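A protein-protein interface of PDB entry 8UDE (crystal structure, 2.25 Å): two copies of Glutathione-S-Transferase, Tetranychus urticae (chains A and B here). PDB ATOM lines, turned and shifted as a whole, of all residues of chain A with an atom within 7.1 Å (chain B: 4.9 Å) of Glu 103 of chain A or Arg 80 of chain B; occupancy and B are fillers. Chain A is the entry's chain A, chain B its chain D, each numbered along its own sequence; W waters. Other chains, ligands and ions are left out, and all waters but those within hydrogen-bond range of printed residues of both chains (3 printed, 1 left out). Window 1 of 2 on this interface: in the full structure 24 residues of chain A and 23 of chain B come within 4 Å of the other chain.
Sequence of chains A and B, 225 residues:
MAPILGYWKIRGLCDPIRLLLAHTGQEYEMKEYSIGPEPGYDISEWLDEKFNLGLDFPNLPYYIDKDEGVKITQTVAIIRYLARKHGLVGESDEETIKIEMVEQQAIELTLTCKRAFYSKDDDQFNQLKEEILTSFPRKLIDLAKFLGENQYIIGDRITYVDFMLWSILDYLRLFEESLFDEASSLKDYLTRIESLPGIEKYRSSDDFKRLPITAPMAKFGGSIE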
ATOM      1  N   VAL A  76       8.348  19.817 -10.562  1.00  0.00           N
ATOM      2  CA  VAL A  76       9.366  20.181  -9.580  1.00  0.00           C
ATOM      3  C   VAL A  76       9.064  21.565  -8.999  1.00  0.00           C
ATOM      4  O   VAL A  76       9.248  21.801  -7.805  1.00  0.00           O
ATOM      5  CB  VAL A  76      10.773  20.063 -10.205  1.00  0.00           C
ATOM      6  CG1 VAL A  76      11.913  20.611  -9.355  1.00  0.00           C
ATOM      7  CG2 VAL A  76      11.066  18.606 -10.568  1.00  0.00           C
ATOM      8  N   ILE A  79       6.340  20.968  -6.514  1.00  0.00           N
ATOM      9  CA  ILE A  79       6.659  20.228  -5.312  1.00  0.00           C
ATOM     10  C   ILE A  79       7.538  21.090  -4.415  1.00  0.00           C
ATOM     11  O   ILE A  79       7.477  20.937  -3.184  1.00  0.00           O
ATOM     12  CB  ILE A  79       7.286  18.835  -5.550  1.00  0.00           C
ATOM     13  CG1 ILE A  79       7.117  17.976  -4.288  1.00  0.00           C
ATOM     14  CG2 ILE A  79       8.738  18.921  -5.948  1.00  0.00           C
ATOM     15  CD1 ILE A  79       7.538  16.532  -4.405  1.00  0.00           C
ATOM     16  N   ARG A  80       8.347  21.985  -5.008  1.00  0.00           N
ATOM     17  CA  ARG A  80       9.203  22.848  -4.195  1.00  0.00           C
ATOM     18  C   ARG A  80       8.342  23.908  -3.508  1.00  0.00           C
ATOM     19  O   ARG A  80       8.586  24.238  -2.371  1.00  0.00           O
ATOM     20  CB  ARG A  80      10.332  23.510  -5.010  1.00  0.00           C
ATOM     21  CG  ARG A  80      11.480  22.574  -5.367  1.00  0.00           C
ATOM     22  CD  ARG A  80      12.539  23.102  -6.321  1.00  0.00           C
ATOM     23  NE  ARG A  80      13.291  24.275  -5.909  1.00  0.00           N
ATOM     24  CZ  ARG A  80      14.365  24.287  -5.117  1.00  0.00           C
ATOM     25  NH1 ARG A  80      14.644  23.249  -4.344  1.00  0.00           N
ATOM     26  NH2 ARG A  80      15.137  25.362  -5.064  1.00  0.00           N
ATOM     27  N   ASP A  93      22.171  25.626   4.566  1.00  0.00           N
ATOM     28  CA  ASP A  93      22.674  25.538   3.205  1.00  0.00           C
ATOM     29  C   ASP A  93      23.227  24.132   2.989  1.00  0.00           C
ATOM     30  O   ASP A  93      23.069  23.583   1.931  1.00  0.00           O
ATOM     31  CB  ASP A  93      23.715  26.637   2.879  1.00  0.00           C
ATOM     32  CG  ASP A  93      23.881  26.909   1.382  1.00  0.00           C
ATOM     33  OD1 ASP A  93      22.855  26.889   0.684  1.00  0.00           O
ATOM     34  OD2 ASP A  93      25.025  27.135   0.917  1.00  0.00           O
ATOM     35  N   THR A  96      20.454  21.885   2.210  1.00  0.00           N
ATOM     36  CA  THR A  96      19.880  22.255   0.922  1.00  0.00           C
ATOM     37  C   THR A  96      20.723  21.693  -0.211  1.00  0.00           C
ATOM     38  O   THR A  96      20.173  21.177  -1.172  1.00  0.00           O
ATOM     39  CB  THR A  96      19.703  23.773   0.809  1.00  0.00           C
ATOM     40  OG1 THR A  96      18.671  24.122   1.719  1.00  0.00           O
ATOM     41  CG2 THR A  96      19.328  24.260  -0.572  1.00  0.00           C
ATOM     42  N   ILE A  97      22.048  21.791  -0.093  1.00  0.00           N
ATOM     43  CA  ILE A  97      22.952  21.235  -1.090  1.00  0.00           C
ATOM     44  C   ILE A  97      22.692  19.725  -1.240  1.00  0.00           C
ATOM     45  O   ILE A  97      22.610  19.184  -2.344  1.00  0.00           O
ATOM     46  CB  ILE A  97      24.417  21.487  -0.701  1.00  0.00           C
ATOM     47  CG1 ILE A  97      24.780  22.972  -0.709  1.00  0.00           C
ATOM     48  CG2 ILE A  97      25.329  20.679  -1.613  1.00  0.00           C
ATOM     49  CD1 ILE A  97      26.060  23.300  -0.015  1.00  0.00           C
ATOM     50  N   LYS A  98      22.569  19.018  -0.113  1.00  0.00           N
ATOM     51  CA  LYS A  98      22.347  17.581  -0.189  1.00  0.00           C
ATOM     52  C   LYS A  98      21.002  17.285  -0.831  1.00  0.00           C
ATOM     53  O   LYS A  98      20.905  16.397  -1.650  1.00  0.00           O
ATOM     54  CB  LYS A  98      22.381  16.942   1.190  1.00  0.00           C
ATOM     55  CG  LYS A  98      23.722  16.941   1.882  1.00  0.00           C
ATOM     56  CD  LYS A  98      23.578  16.399   3.327  1.00  0.00           C
ATOM     57  CE  LYS A  98      24.801  16.658   4.186  1.00  0.00           C
ATOM     58  NZ  LYS A  98      24.658  15.993   5.493  1.00  0.00           N
ATOM     59  N   ILE A  99      19.968  18.012  -0.441  1.00  0.00           N
ATOM     60  CA  ILE A  99      18.647  17.811  -0.995  1.00  0.00           C
ATOM     61  C   ILE A  99      18.678  18.020  -2.507  1.00  0.00           C
ATOM     62  O   ILE A  99      18.064  17.265  -3.261  1.00  0.00           O
ATOM     63  CB  ILE A  99      17.638  18.774  -0.337  1.00  0.00           C
ATOM     64  CG1 ILE A  99      17.369  18.443   1.124  1.00  0.00           C
ATOM     65  CG2 ILE A  99      16.336  18.824  -1.113  1.00  0.00           C
ATOM     66  CD1 ILE A  99      16.646  19.577   1.808  1.00  0.00           C
ATOM     67  N   GLU A 100      19.396  19.044  -2.961  1.00  0.00           N
ATOM     68  CA  GLU A 100      19.317  19.403  -4.361  1.00  0.00           C
ATOM     69  C   GLU A 100      20.172  18.457  -5.194  1.00  0.00           C
ATOM     70  O   GLU A 100      19.792  18.183  -6.329  1.00  0.00           O
ATOM     71  CB  GLU A 100      19.626  20.886  -4.523  1.00  0.00           C
ATOM     72  CG  GLU A 100      18.522  21.729  -3.877  1.00  0.00           C
ATOM     73  CD  GLU A 100      18.745  23.243  -3.926  1.00  0.00           C
ATOM     74  OE1 GLU A 100      19.884  23.672  -4.307  1.00  0.00           O
ATOM     75  OE2 GLU A 100      17.779  23.997  -3.633  1.00  0.00           O
ATOM     76  N   MET A 101      21.271  17.903  -4.629  1.00  0.00           N
ATOM     77  CA  MET A 101      22.044  16.910  -5.375  1.00  0.00           C
ATOM     78  C   MET A 101      21.145  15.698  -5.590  1.00  0.00           C
ATOM     79  O   MET A 101      21.033  15.195  -6.706  1.00  0.00           O
ATOM     80  CB  MET A 101      23.353  16.469  -4.699  1.00  0.00           C
ATOM     81  CG  MET A 101      24.486  17.459  -4.797  1.00  0.00           C
ATOM     82  SD  MET A 101      26.140  16.833  -4.241  1.00  0.00           S
ATOM     83  CE  MET A 101      25.847  16.439  -2.511  1.00  0.00           C
ATOM     84  N   VAL A 102      20.470  15.232  -4.534  1.00  0.00           N
ATOM     85  CA  VAL A 102      19.663  14.031  -4.641  1.00  0.00           C
ATOM     86  C   VAL A 102      18.485  14.306  -5.567  1.00  0.00           C
ATOM     87  O   VAL A 102      18.059  13.420  -6.311  1.00  0.00           O
ATOM     88  CB  VAL A 102      19.239  13.563  -3.242  1.00  0.00           C
ATOM     89  CG1 VAL A 102      18.219  12.438  -3.292  1.00  0.00           C
ATOM     90  CG2 VAL A 102      20.476  13.144  -2.436  1.00  0.00           C
ATOM     91  N   GLU A 103      17.980  15.540  -5.551  1.00  0.00           N
ATOM     92  CA  GLU A 103      16.823  15.925  -6.346  1.00  0.00           C
ATOM     93  C   GLU A 103      17.140  15.744  -7.827  1.00  0.00           C
ATOM     94  O   GLU A 103      16.304  15.220  -8.557  1.00  0.00           O
ATOM     95  CB  GLU A 103      16.436  17.375  -6.033  1.00  0.00           C
ATOM     96  CG  GLU A 103      15.367  17.958  -6.933  1.00  0.00           C
ATOM     97  CD  GLU A 103      15.307  19.474  -7.004  1.00  0.00           C
ATOM     98  OE1 GLU A 103      14.887  20.089  -6.040  1.00  0.00           O
ATOM     99  OE2 GLU A 103      15.755  20.023  -7.978  1.00  0.00           O
ATOM    100  N   GLN A 104      18.337  16.168  -8.256  1.00  0.00           N
ATOM    101  CA  GLN A 104      18.736  16.035  -9.649  1.00  0.00           C
ATOM    102  C   GLN A 104      18.942  14.567 -10.024  1.00  0.00           C
ATOM    103  O   GLN A 104      18.669  14.165 -11.152  1.00  0.00           O
ATOM    104  CB  GLN A 104      19.973  16.858  -9.915  1.00  0.00           C
ATOM    105  CG  GLN A 104      19.718  18.351  -9.692  1.00  0.00           C
ATOM    106  CD  GLN A 104      18.649  18.862 -10.633  1.00  0.00           C
ATOM    107  OE1 GLN A 104      18.800  18.832 -11.863  1.00  0.00           O
ATOM    108  NE2 GLN A 104      17.598  19.422 -10.055  1.00  0.00           N
ATOM    109  N   GLN A 105      19.428  13.775  -9.070  1.00  0.00           N
ATOM    110  CA  GLN A 105      19.571  12.320  -9.326  1.00  0.00           C
ATOM    111  C   GLN A 105      18.172  11.730  -9.519  1.00  0.00           C
ATOM    112  O   GLN A 105      18.009  10.897 -10.427  1.00  0.00           O
ATOM    113  CB  GLN A 105      20.306  11.645  -8.167  1.00  0.00           C
ATOM    114  CG  GLN A 105      21.795  11.952  -8.124  1.00  0.00           C
ATOM    115  CD  GLN A 105      22.539  11.218  -9.211  1.00  0.00           C
ATOM    116  OE1 GLN A 105      22.530   9.991  -9.275  1.00  0.00           O
ATOM    117  NE2 GLN A 105      23.189  11.971 -10.084  1.00  0.00           N
ATOM    118  N   ALA A 106      17.199  12.170  -8.716  1.00  0.00           N
ATOM    119  CA  ALA A 106      15.870  11.593  -8.796  1.00  0.00           C
ATOM    120  C   ALA A 106      15.241  11.977 -10.128  1.00  0.00           C
ATOM    121  O   ALA A 106      14.587  11.168 -10.774  1.00  0.00           O
ATOM    122  CB  ALA A 106      15.013  12.046  -7.630  1.00  0.00           C
ATOM    123  N   ILE A 107      15.440  13.232 -10.531  1.00  0.00           N
ATOM    124  CA  ILE A 107      14.928  13.730 -11.790  1.00  0.00           C
ATOM    125  C   ILE A 107      15.525  12.932 -12.943  1.00  0.00           C
ATOM    126  O   ILE A 107      14.779  12.608 -13.851  1.00  0.00           O
ATOM    127  CB  ILE A 107      15.165  15.239 -11.946  1.00  0.00           C
ATOM    128  CG1 ILE A 107      14.273  16.017 -10.967  1.00  0.00           C
ATOM    129  CG2 ILE A 107      14.965  15.675 -13.397  1.00  0.00           C
ATOM    130  CD1 ILE A 107      14.616  17.518 -10.897  1.00  0.00           C
ATOM    131  N   GLU A 108      16.826  12.618 -12.909  1.00  0.00           N
ATOM    132  CA  GLU A 108      17.453  11.914 -14.020  1.00  0.00           C
ATOM    133  C   GLU A 108      16.841  10.521 -14.137  1.00  0.00           C
ATOM    134  O   GLU A 108      16.470  10.118 -15.228  1.00  0.00           O
ATOM    135  CB  GLU A 108      18.974  11.885 -13.876  1.00  0.00           C
ATOM    136  CG  GLU A 108      19.624  13.253 -14.120  1.00  0.00           C
ATOM    137  CD  GLU A 108      21.148  13.308 -14.048  1.00  0.00           C
ATOM    138  OE1 GLU A 108      21.796  12.237 -13.932  1.00  0.00           O
ATOM    139  OE2 GLU A 108      21.695  14.430 -14.070  1.00  0.00           O
ATOM    140  N   LEU A 109      16.739   9.796 -13.015  1.00  0.00           N
ATOM    141  CA  LEU A 109      16.114   8.482 -12.985  1.00  0.00           C
ATOM    142  C   LEU A 109      14.712   8.553 -13.599  1.00  0.00           C
ATOM    143  O   LEU A 109      14.331   7.706 -14.411  1.00  0.00           O
ATOM    144  CB  LEU A 109      16.028   7.978 -11.533  1.00  0.00           C
ATOM    145  CG  LEU A 109      17.345   7.759 -10.787  1.00  0.00           C
ATOM    146  CD1 LEU A 109      17.113   7.149  -9.415  1.00  0.00           C
ATOM    147  CD2 LEU A 109      18.276   6.880 -11.587  1.00  0.00           C
ATOM    148  N   THR A 110      13.950   9.572 -13.186  1.00  0.00           N
ATOM    149  CA  THR A 110      12.550   9.711 -13.548  1.00  0.00           C
ATOM    150  C   THR A 110      12.405   9.956 -15.046  1.00  0.00           C
ATOM    151  O   THR A 110      11.579   9.305 -15.706  1.00  0.00           O
ATOM    152  CB  THR A 110      11.890  10.803 -12.685  1.00  0.00           C
ATOM    153  OG1 THR A 110      12.044  10.412 -11.329  1.00  0.00           O
ATOM    154  CG2 THR A 110      10.414  10.995 -12.945  1.00  0.00           C
ATOM    155  N   ILE A 153      17.042  11.248   3.472  1.00  0.00           N
ATOM    156  CA  ILE A 153      18.197  11.745   2.726  1.00  0.00           C
ATOM    157  C   ILE A 153      19.088  12.638   3.568  1.00  0.00           C
ATOM    158  O   ILE A 153      20.284  12.479   3.543  1.00  0.00           O
ATOM    159  CB  ILE A 153      17.670  12.466   1.453  1.00  0.00           C
ATOM    160  CG1 ILE A 153      17.171  11.441   0.449  1.00  0.00           C
ATOM    161  CG2 ILE A 153      18.702  13.413   0.821  1.00  0.00           C
ATOM    162  CD1 ILE A 153      18.293  10.501   0.037  1.00  0.00           C
ATOM    163  N   TYR A 160      11.266  17.022   0.875  1.00  0.00           N
ATOM    164  CA  TYR A 160      10.443  16.783  -0.294  1.00  0.00           C
ATOM    165  C   TYR A 160      11.098  15.742  -1.195  1.00  0.00           C
ATOM    166  O   TYR A 160      10.382  14.986  -1.852  1.00  0.00           O
ATOM    167  CB  TYR A 160      10.126  18.053  -1.070  1.00  0.00           C
ATOM    168  CG  TYR A 160      11.303  18.712  -1.766  1.00  0.00           C
ATOM    169  CD1 TYR A 160      11.589  18.432  -3.101  1.00  0.00           C
ATOM    170  CD2 TYR A 160      12.068  19.673  -1.116  1.00  0.00           C
ATOM    171  CE1 TYR A 160      12.633  19.054  -3.753  1.00  0.00           C
ATOM    172  CE2 TYR A 160      13.147  20.254  -1.742  1.00  0.00           C
ATOM    173  CZ  TYR A 160      13.411  19.972  -3.075  1.00  0.00           C
ATOM    174  OH  TYR A 160      14.442  20.617  -3.717  1.00  0.00           O
ATOM    175  N   VAL A 161      12.439  15.701  -1.214  1.00  0.00           N
ATOM    176  CA  VAL A 161      13.141  14.823  -2.134  1.00  0.00           C
ATOM    177  C   VAL A 161      12.903  13.355  -1.777  1.00  0.00           C
ATOM    178  O   VAL A 161      13.047  12.507  -2.650  1.00  0.00           O
ATOM    179  CB  VAL A 161      14.645  15.114  -2.258  1.00  0.00           C
ATOM    180  CG1 VAL A 161      14.908  16.380  -3.028  1.00  0.00           C
ATOM    181  CG2 VAL A 161      15.350  15.122  -0.916  1.00  0.00           C
ATOM    182  N   MET A 164      10.174  12.353  -3.946  1.00  0.00           N
ATOM    183  CA  MET A 164      10.619  12.188  -5.346  1.00  0.00           C
ATOM    184  C   MET A 164      11.397  10.878  -5.501  1.00  0.00           C
ATOM    185  O   MET A 164      11.144  10.096  -6.426  1.00  0.00           O
ATOM    186  CB  MET A 164      11.515  13.348  -5.792  1.00  0.00           C
ATOM    187  CG  MET A 164      10.789  14.708  -5.745  1.00  0.00           C
ATOM    188  SD  MET A 164      11.844  16.113  -6.063  1.00  0.00           S
ATOM    189  CE  MET A 164      12.193  15.789  -7.789  1.00  0.00           C
ATOM    190  N   VAL B  76      22.747  21.608 -11.615  1.00  0.00           N
ATOM    191  CA  VAL B  76      21.698  22.463 -11.092  1.00  0.00           C
ATOM    192  C   VAL B  76      21.932  22.717  -9.590  1.00  0.00           C
ATOM    193  O   VAL B  76      21.716  23.818  -9.106  1.00  0.00           O
ATOM    194  CB  VAL B  76      20.318  21.855 -11.404  1.00  0.00           C
ATOM    195  CG1 VAL B  76      19.174  22.626 -10.739  1.00  0.00           C
ATOM    196  CG2 VAL B  76      20.080  21.783 -12.912  1.00  0.00           C
ATOM    197  N   ALA B  77      22.453  21.739  -8.852  1.00  0.00           N
ATOM    198  CA  ALA B  77      22.738  21.956  -7.443  1.00  0.00           C
ATOM    199  C   ALA B  77      23.888  22.935  -7.319  1.00  0.00           C
ATOM    200  O   ALA B  77      23.859  23.779  -6.437  1.00  0.00           O
ATOM    201  CB  ALA B  77      23.032  20.685  -6.718  1.00  0.00           C
ATOM    202  N   ILE B  78      24.854  22.866  -8.235  1.00  0.00           N
ATOM    203  CA  ILE B  78      25.970  23.781  -8.215  1.00  0.00           C
ATOM    204  C   ILE B  78      25.442  25.163  -8.472  1.00  0.00           C
ATOM    205  O   ILE B  78      25.868  26.106  -7.807  1.00  0.00           O
ATOM    206  CB  ILE B  78      27.066  23.411  -9.235  1.00  0.00           C
ATOM    207  CG1 ILE B  78      27.681  22.044  -8.910  1.00  0.00           C
ATOM    208  CG2 ILE B  78      28.141  24.491  -9.282  1.00  0.00           C
ATOM    209  CD1 ILE B  78      28.564  21.458 -10.027  1.00  0.00           C
ATOM    210  N   ILE B  79      24.590  25.298  -9.499  1.00  0.00           N
ATOM    211  CA  ILE B  79      24.239  26.635  -9.943  1.00  0.00           C
ATOM    212  C   ILE B  79      23.339  27.290  -8.903  1.00  0.00           C
ATOM    213  O   ILE B  79      23.400  28.505  -8.760  1.00  0.00           O
ATOM    214  CB  ILE B  79      23.641  26.705 -11.362  1.00  0.00           C
ATOM    215  CG1 ILE B  79      23.768  28.118 -11.912  1.00  0.00           C
ATOM    216  CG2 ILE B  79      22.202  26.319 -11.388  1.00  0.00           C
ATOM    217  CD1 ILE B  79      23.484  28.278 -13.395  1.00  0.00           C
ATOM    218  N   ARG B  80      22.534  26.492  -8.177  1.00  0.00           N
ATOM    219  CA  ARG B  80      21.636  27.057  -7.177  1.00  0.00           C
ATOM    220  C   ARG B  80      22.468  27.485  -5.984  1.00  0.00           C
ATOM    221  O   ARG B  80      22.192  28.514  -5.395  1.00  0.00           O
ATOM    222  CB  ARG B  80      20.494  26.117  -6.748  1.00  0.00           C
ATOM    223  CG  ARG B  80      19.383  25.897  -7.784  1.00  0.00           C
ATOM    224  CD  ARG B  80      18.208  25.109  -7.213  1.00  0.00           C
ATOM    225  NE  ARG B  80      17.258  24.492  -8.108  1.00  0.00           N
ATOM    226  CZ  ARG B  80      16.756  23.251  -7.967  1.00  0.00           C
ATOM    227  NH1 ARG B  80      17.276  22.416  -7.080  1.00  0.00           N
ATOM    228  NH2 ARG B  80      15.748  22.817  -8.720  1.00  0.00           N
ATOM    229  N   TYR B  81      23.441  26.647  -5.590  1.00  0.00           N
ATOM    230  CA  TYR B  81      24.397  27.010  -4.554  1.00  0.00           C
ATOM    231  C   TYR B  81      24.997  28.383  -4.864  1.00  0.00           C
ATOM    232  O   TYR B  81      24.960  29.264  -4.016  1.00  0.00           O
ATOM    233  CB  TYR B  81      25.497  25.952  -4.401  1.00  0.00           C
ATOM    234  CG  TYR B  81      26.661  26.430  -3.533  1.00  0.00           C
ATOM    235  CD1 TYR B  81      26.609  26.433  -2.143  1.00  0.00           C
ATOM    236  CD2 TYR B  81      27.797  26.936  -4.127  1.00  0.00           C
ATOM    237  CE1 TYR B  81      27.649  26.920  -1.372  1.00  0.00           C
ATOM    238  CE2 TYR B  81      28.853  27.392  -3.370  1.00  0.00           C
ATOM    239  CZ  TYR B  81      28.777  27.393  -1.992  1.00  0.00           C
ATOM    240  OH  TYR B  81      29.854  27.857  -1.316  1.00  0.00           O
ATOM    241  N   LEU B  82      25.538  28.554  -6.074  1.00  0.00           N
ATOM    242  CA  LEU B  82      26.189  29.808  -6.476  1.00  0.00           C
ATOM    243  C   LEU B  82      25.178  30.941  -6.536  1.00  0.00           C
ATOM    244  O   LEU B  82      25.475  32.046  -6.151  1.00  0.00           O
ATOM    245  CB  LEU B  82      26.861  29.629  -7.840  1.00  0.00           C
ATOM    246  CG  LEU B  82      28.043  28.680  -7.858  1.00  0.00           C
ATOM    247  CD1 LEU B  82      28.488  28.378  -9.274  1.00  0.00           C
ATOM    248  CD2 LEU B  82      29.172  29.267  -7.040  1.00  0.00           C
ATOM    249  N   ALA B  83      23.961  30.656  -6.975  1.00  0.00           N
ATOM    250  CA  ALA B  83      22.937  31.683  -7.020  1.00  0.00           C
ATOM    251  C   ALA B  83      22.651  32.224  -5.625  1.00  0.00           C
ATOM    252  O   ALA B  83      22.584  33.441  -5.444  1.00  0.00           O
ATOM    253  CB  ALA B  83      21.701  31.130  -7.662  1.00  0.00           C
ATOM    254  N   ARG B  84      22.489  31.327  -4.632  1.00  0.00           N
ATOM    255  CA  ARG B  84      22.180  31.793  -3.291  1.00  0.00           C
ATOM    256  C   ARG B  84      23.350  32.634  -2.752  1.00  0.00           C
ATOM    257  O   ARG B  84      23.140  33.661  -2.139  1.00  0.00           O
ATOM    258  CB  ARG B  84      21.816  30.613  -2.378  1.00  0.00           C
ATOM    259  CG  ARG B  84      20.600  29.800  -2.804  1.00  0.00           C
ATOM    260  CD  ARG B  84      20.244  28.774  -1.723  1.00  0.00           C
ATOM    261  NE  ARG B  84      21.288  27.754  -1.574  1.00  0.00           N
ATOM    262  CZ  ARG B  84      21.407  26.634  -2.305  1.00  0.00           C
ATOM    263  NH1 ARG B  84      20.537  26.356  -3.248  1.00  0.00           N
ATOM    264  NH2 ARG B  84      22.384  25.776  -2.066  1.00  0.00           N
ATOM    265  N   GLU B 103      13.097  27.145 -14.983  1.00  0.00           N
ATOM    266  CA  GLU B 103      14.224  26.264 -14.718  1.00  0.00           C
ATOM    267  C   GLU B 103      13.975  24.847 -15.259  1.00  0.00           C
ATOM    268  O   GLU B 103      14.851  24.274 -15.923  1.00  0.00           O
ATOM    269  CB  GLU B 103      14.496  26.198 -13.220  1.00  0.00           C
ATOM    270  CG  GLU B 103      15.649  25.307 -12.823  1.00  0.00           C
ATOM    271  CD  GLU B 103      15.632  24.917 -11.348  1.00  0.00           C
ATOM    272  OE1 GLU B 103      15.939  25.753 -10.524  1.00  0.00           O
ATOM    273  OE2 GLU B 103      15.290  23.763 -11.045  1.00  0.00           O
ATOM    274  N   GLN B 104      12.784  24.331 -15.020  1.00  0.00           N
ATOM    275  CA  GLN B 104      12.412  23.010 -15.482  1.00  0.00           C
ATOM    276  C   GLN B 104      12.293  22.976 -17.013  1.00  0.00           C
ATOM    277  O   GLN B 104      12.619  21.961 -17.645  1.00  0.00           O
ATOM    278  CB  GLN B 104      11.120  22.555 -14.818  1.00  0.00           C
ATOM    279  CG  GLN B 104      11.264  22.402 -13.306  1.00  0.00           C
ATOM    280  CD  GLN B 104      12.404  21.497 -12.862  1.00  0.00           C
ATOM    281  OE1 GLN B 104      13.303  21.951 -12.165  1.00  0.00           O
ATOM    282  NE2 GLN B 104      12.386  20.223 -13.239  1.00  0.00           N
ATOM    283  N   TYR B 160      19.624  33.336 -11.768  1.00  0.00           N
ATOM    284  CA  TYR B 160      20.461  32.244 -12.224  1.00  0.00           C
ATOM    285  C   TYR B 160      19.873  31.573 -13.457  1.00  0.00           C
ATOM    286  O   TYR B 160      20.622  31.115 -14.328  1.00  0.00           O
ATOM    287  CB  TYR B 160      20.717  31.208 -11.135  1.00  0.00           C
ATOM    288  CG  TYR B 160      19.540  30.345 -10.729  1.00  0.00           C
ATOM    289  CD1 TYR B 160      18.704  30.722  -9.695  1.00  0.00           C
ATOM    290  CD2 TYR B 160      19.315  29.099 -11.345  1.00  0.00           C
ATOM    291  CE1 TYR B 160      17.637  29.926  -9.314  1.00  0.00           C
ATOM    292  CE2 TYR B 160      18.265  28.291 -10.953  1.00  0.00           C
ATOM    293  CZ  TYR B 160      17.439  28.692  -9.922  1.00  0.00           C
ATOM    294  OH  TYR B 160      16.421  27.879  -9.533  1.00  0.00           O
HETATM  295  O   HOH W   1       9.511  19.758 -13.493  1.00  0.00           O
HETATM  296  O   HOH W   2      24.747  28.668  -1.178  1.00  0.00           O
HETATM  297  O   HOH W   3      22.519  23.314  -4.093  1.00  0.00           O
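NH1 of Arg 80 of chain A sits at hydrogen-bond distance from OH of Tyr 160 of chain A (2.7 Å). The side-chain carboxylate (OE1) of Glu 103 of chain A lies within hydrogen-bond range of the side-chain hydroxyl (OH) of Tyr 160 of chain A. The guanidinium group (NH1) of Arg 84 of chain B lies close to the backbone carbonyl oxygen (O) of Arg 80 of chain B (3.5 Å). OE1 of Gln 104 of chain B sits close to OE2 of Glu 103 of chain B, at 2.9 Å.
Water W2 lies within hydrogen-bond range of the side-chain carboxylate of Asp 93 of chain A and the backbone carbonyl oxygen of Tyr 81 of chain B. Water W3 lies within hydrogen-bond range of OE1 of Glu 100 of chain A, O of Ala 77 of chain B and NH2 of Arg 84 of chain B. Water W1 lies within hydrogen-bond range of the side-chain amide nitrogen of Gln 104 of chain B and the backbone NH of Val 76 of chain A.
Glu 103 of chain A touches one residue of chain B. Of the printed residues of chain A, Tyr 81 of chain B touches Asp 93 and Ile 97. Of the printed residues of chain B, Asp 93 of chain A touches Tyr 81 (3.5 Å) and Arg 84 (2.9 Å). Printed residues of chain A within 4 Å of Val 76 of chain B: Gln 104 (3.4 Å). Printed residues of chain A within 4 Å of Arg 84 of chain B: Asp 93, Thr 96, Ile 97 and Glu 100. Lys 98 of chain A touches none of the printed residues of chain B. Ile 79 of chain A touches none of the printed residues of chain B. The nearest printed residue of chain B that does not touch Glu 103 of chain A is Glu 103 of chain B (4.9 Å). The nearest printed residue of chain B that does not touch Met 101 of chain A is Ile 78 of chain B (6.4 Å).
NE2 of Gln 104 of chain B touches CG2 of Val 76 of chain A (3.4 Å). Arg 80 of chain B touches Arg 80 of chain A (CD to NH2, 3.8 Å). OD2 of Asp 93 of chain A touches CE1 of Tyr 81 of chain B, 3.5 Å away. CG2 of Thr 96 of chain A touches CZ of Arg 84 of chain B, at 3.6 Å. Ile 97 of chain A touches Tyr 81 of chain B. Arg 84 of chain B touches Ile 97 of chain A (NH2 to CG1, 3.9 Å). C of Glu 100 of chain A touches CB of Ala 77 of chain B, 3.9 Å away. CG2 of Val 76 of chain B touches OE1 of Gln 104 of chain A (3.4 Å).
Of the 12 printed residues of chain B, 6 touch a printed residue of chain A. Printed residues of chain B that touch a printed residue of chain A: Val 76, Ala 77, Arg 80, Tyr 81, Arg 84 and Gln 104. Hydrophobic or aromatic side chains of chain B within 4 Å of the printed part of chain A: Val 76, Ala 77 and Tyr 81. Among the printed residues, 13 pairs touch across the chains.
The side-chain carboxylate (OD1) of Asp 93 of chain A lies within salt-bridge range of the guanidinium group (NE) of Arg 84 of chain B (2.9 Å). The side-chain carboxylate (OE2) of Glu 100 of chain A is in salt-bridge range of the guanidinium group (NH1) of Arg 80 of chain B, at 3.8 Å. OE1 of Glu 100 of chain A is in salt-bridge range of NH1 of Arg 84 of chain B, at 3.0 Å. OE2 of Glu 103 of chain A lies within salt-bridge range of NH2 of Arg 80 of chain B.
Val 76 of chain A touches Gln 104 of chain B, and with the chains exchanged Gln 104 of chain A touches Val 76 of chain B. Arg 80 of chain B touches its own counterpart, Arg 80 of chain A. Glu 103 of chain A touches Arg 80 of chain B, but with the chains exchanged Arg 80 of chain A does not touch Glu 103 of chain B (5.5 Å). 6 positions are printed for both chains. Of the 13 pairs that touch across the chains among the printed residues, 3 have their exchanged pair printed and touching as well.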
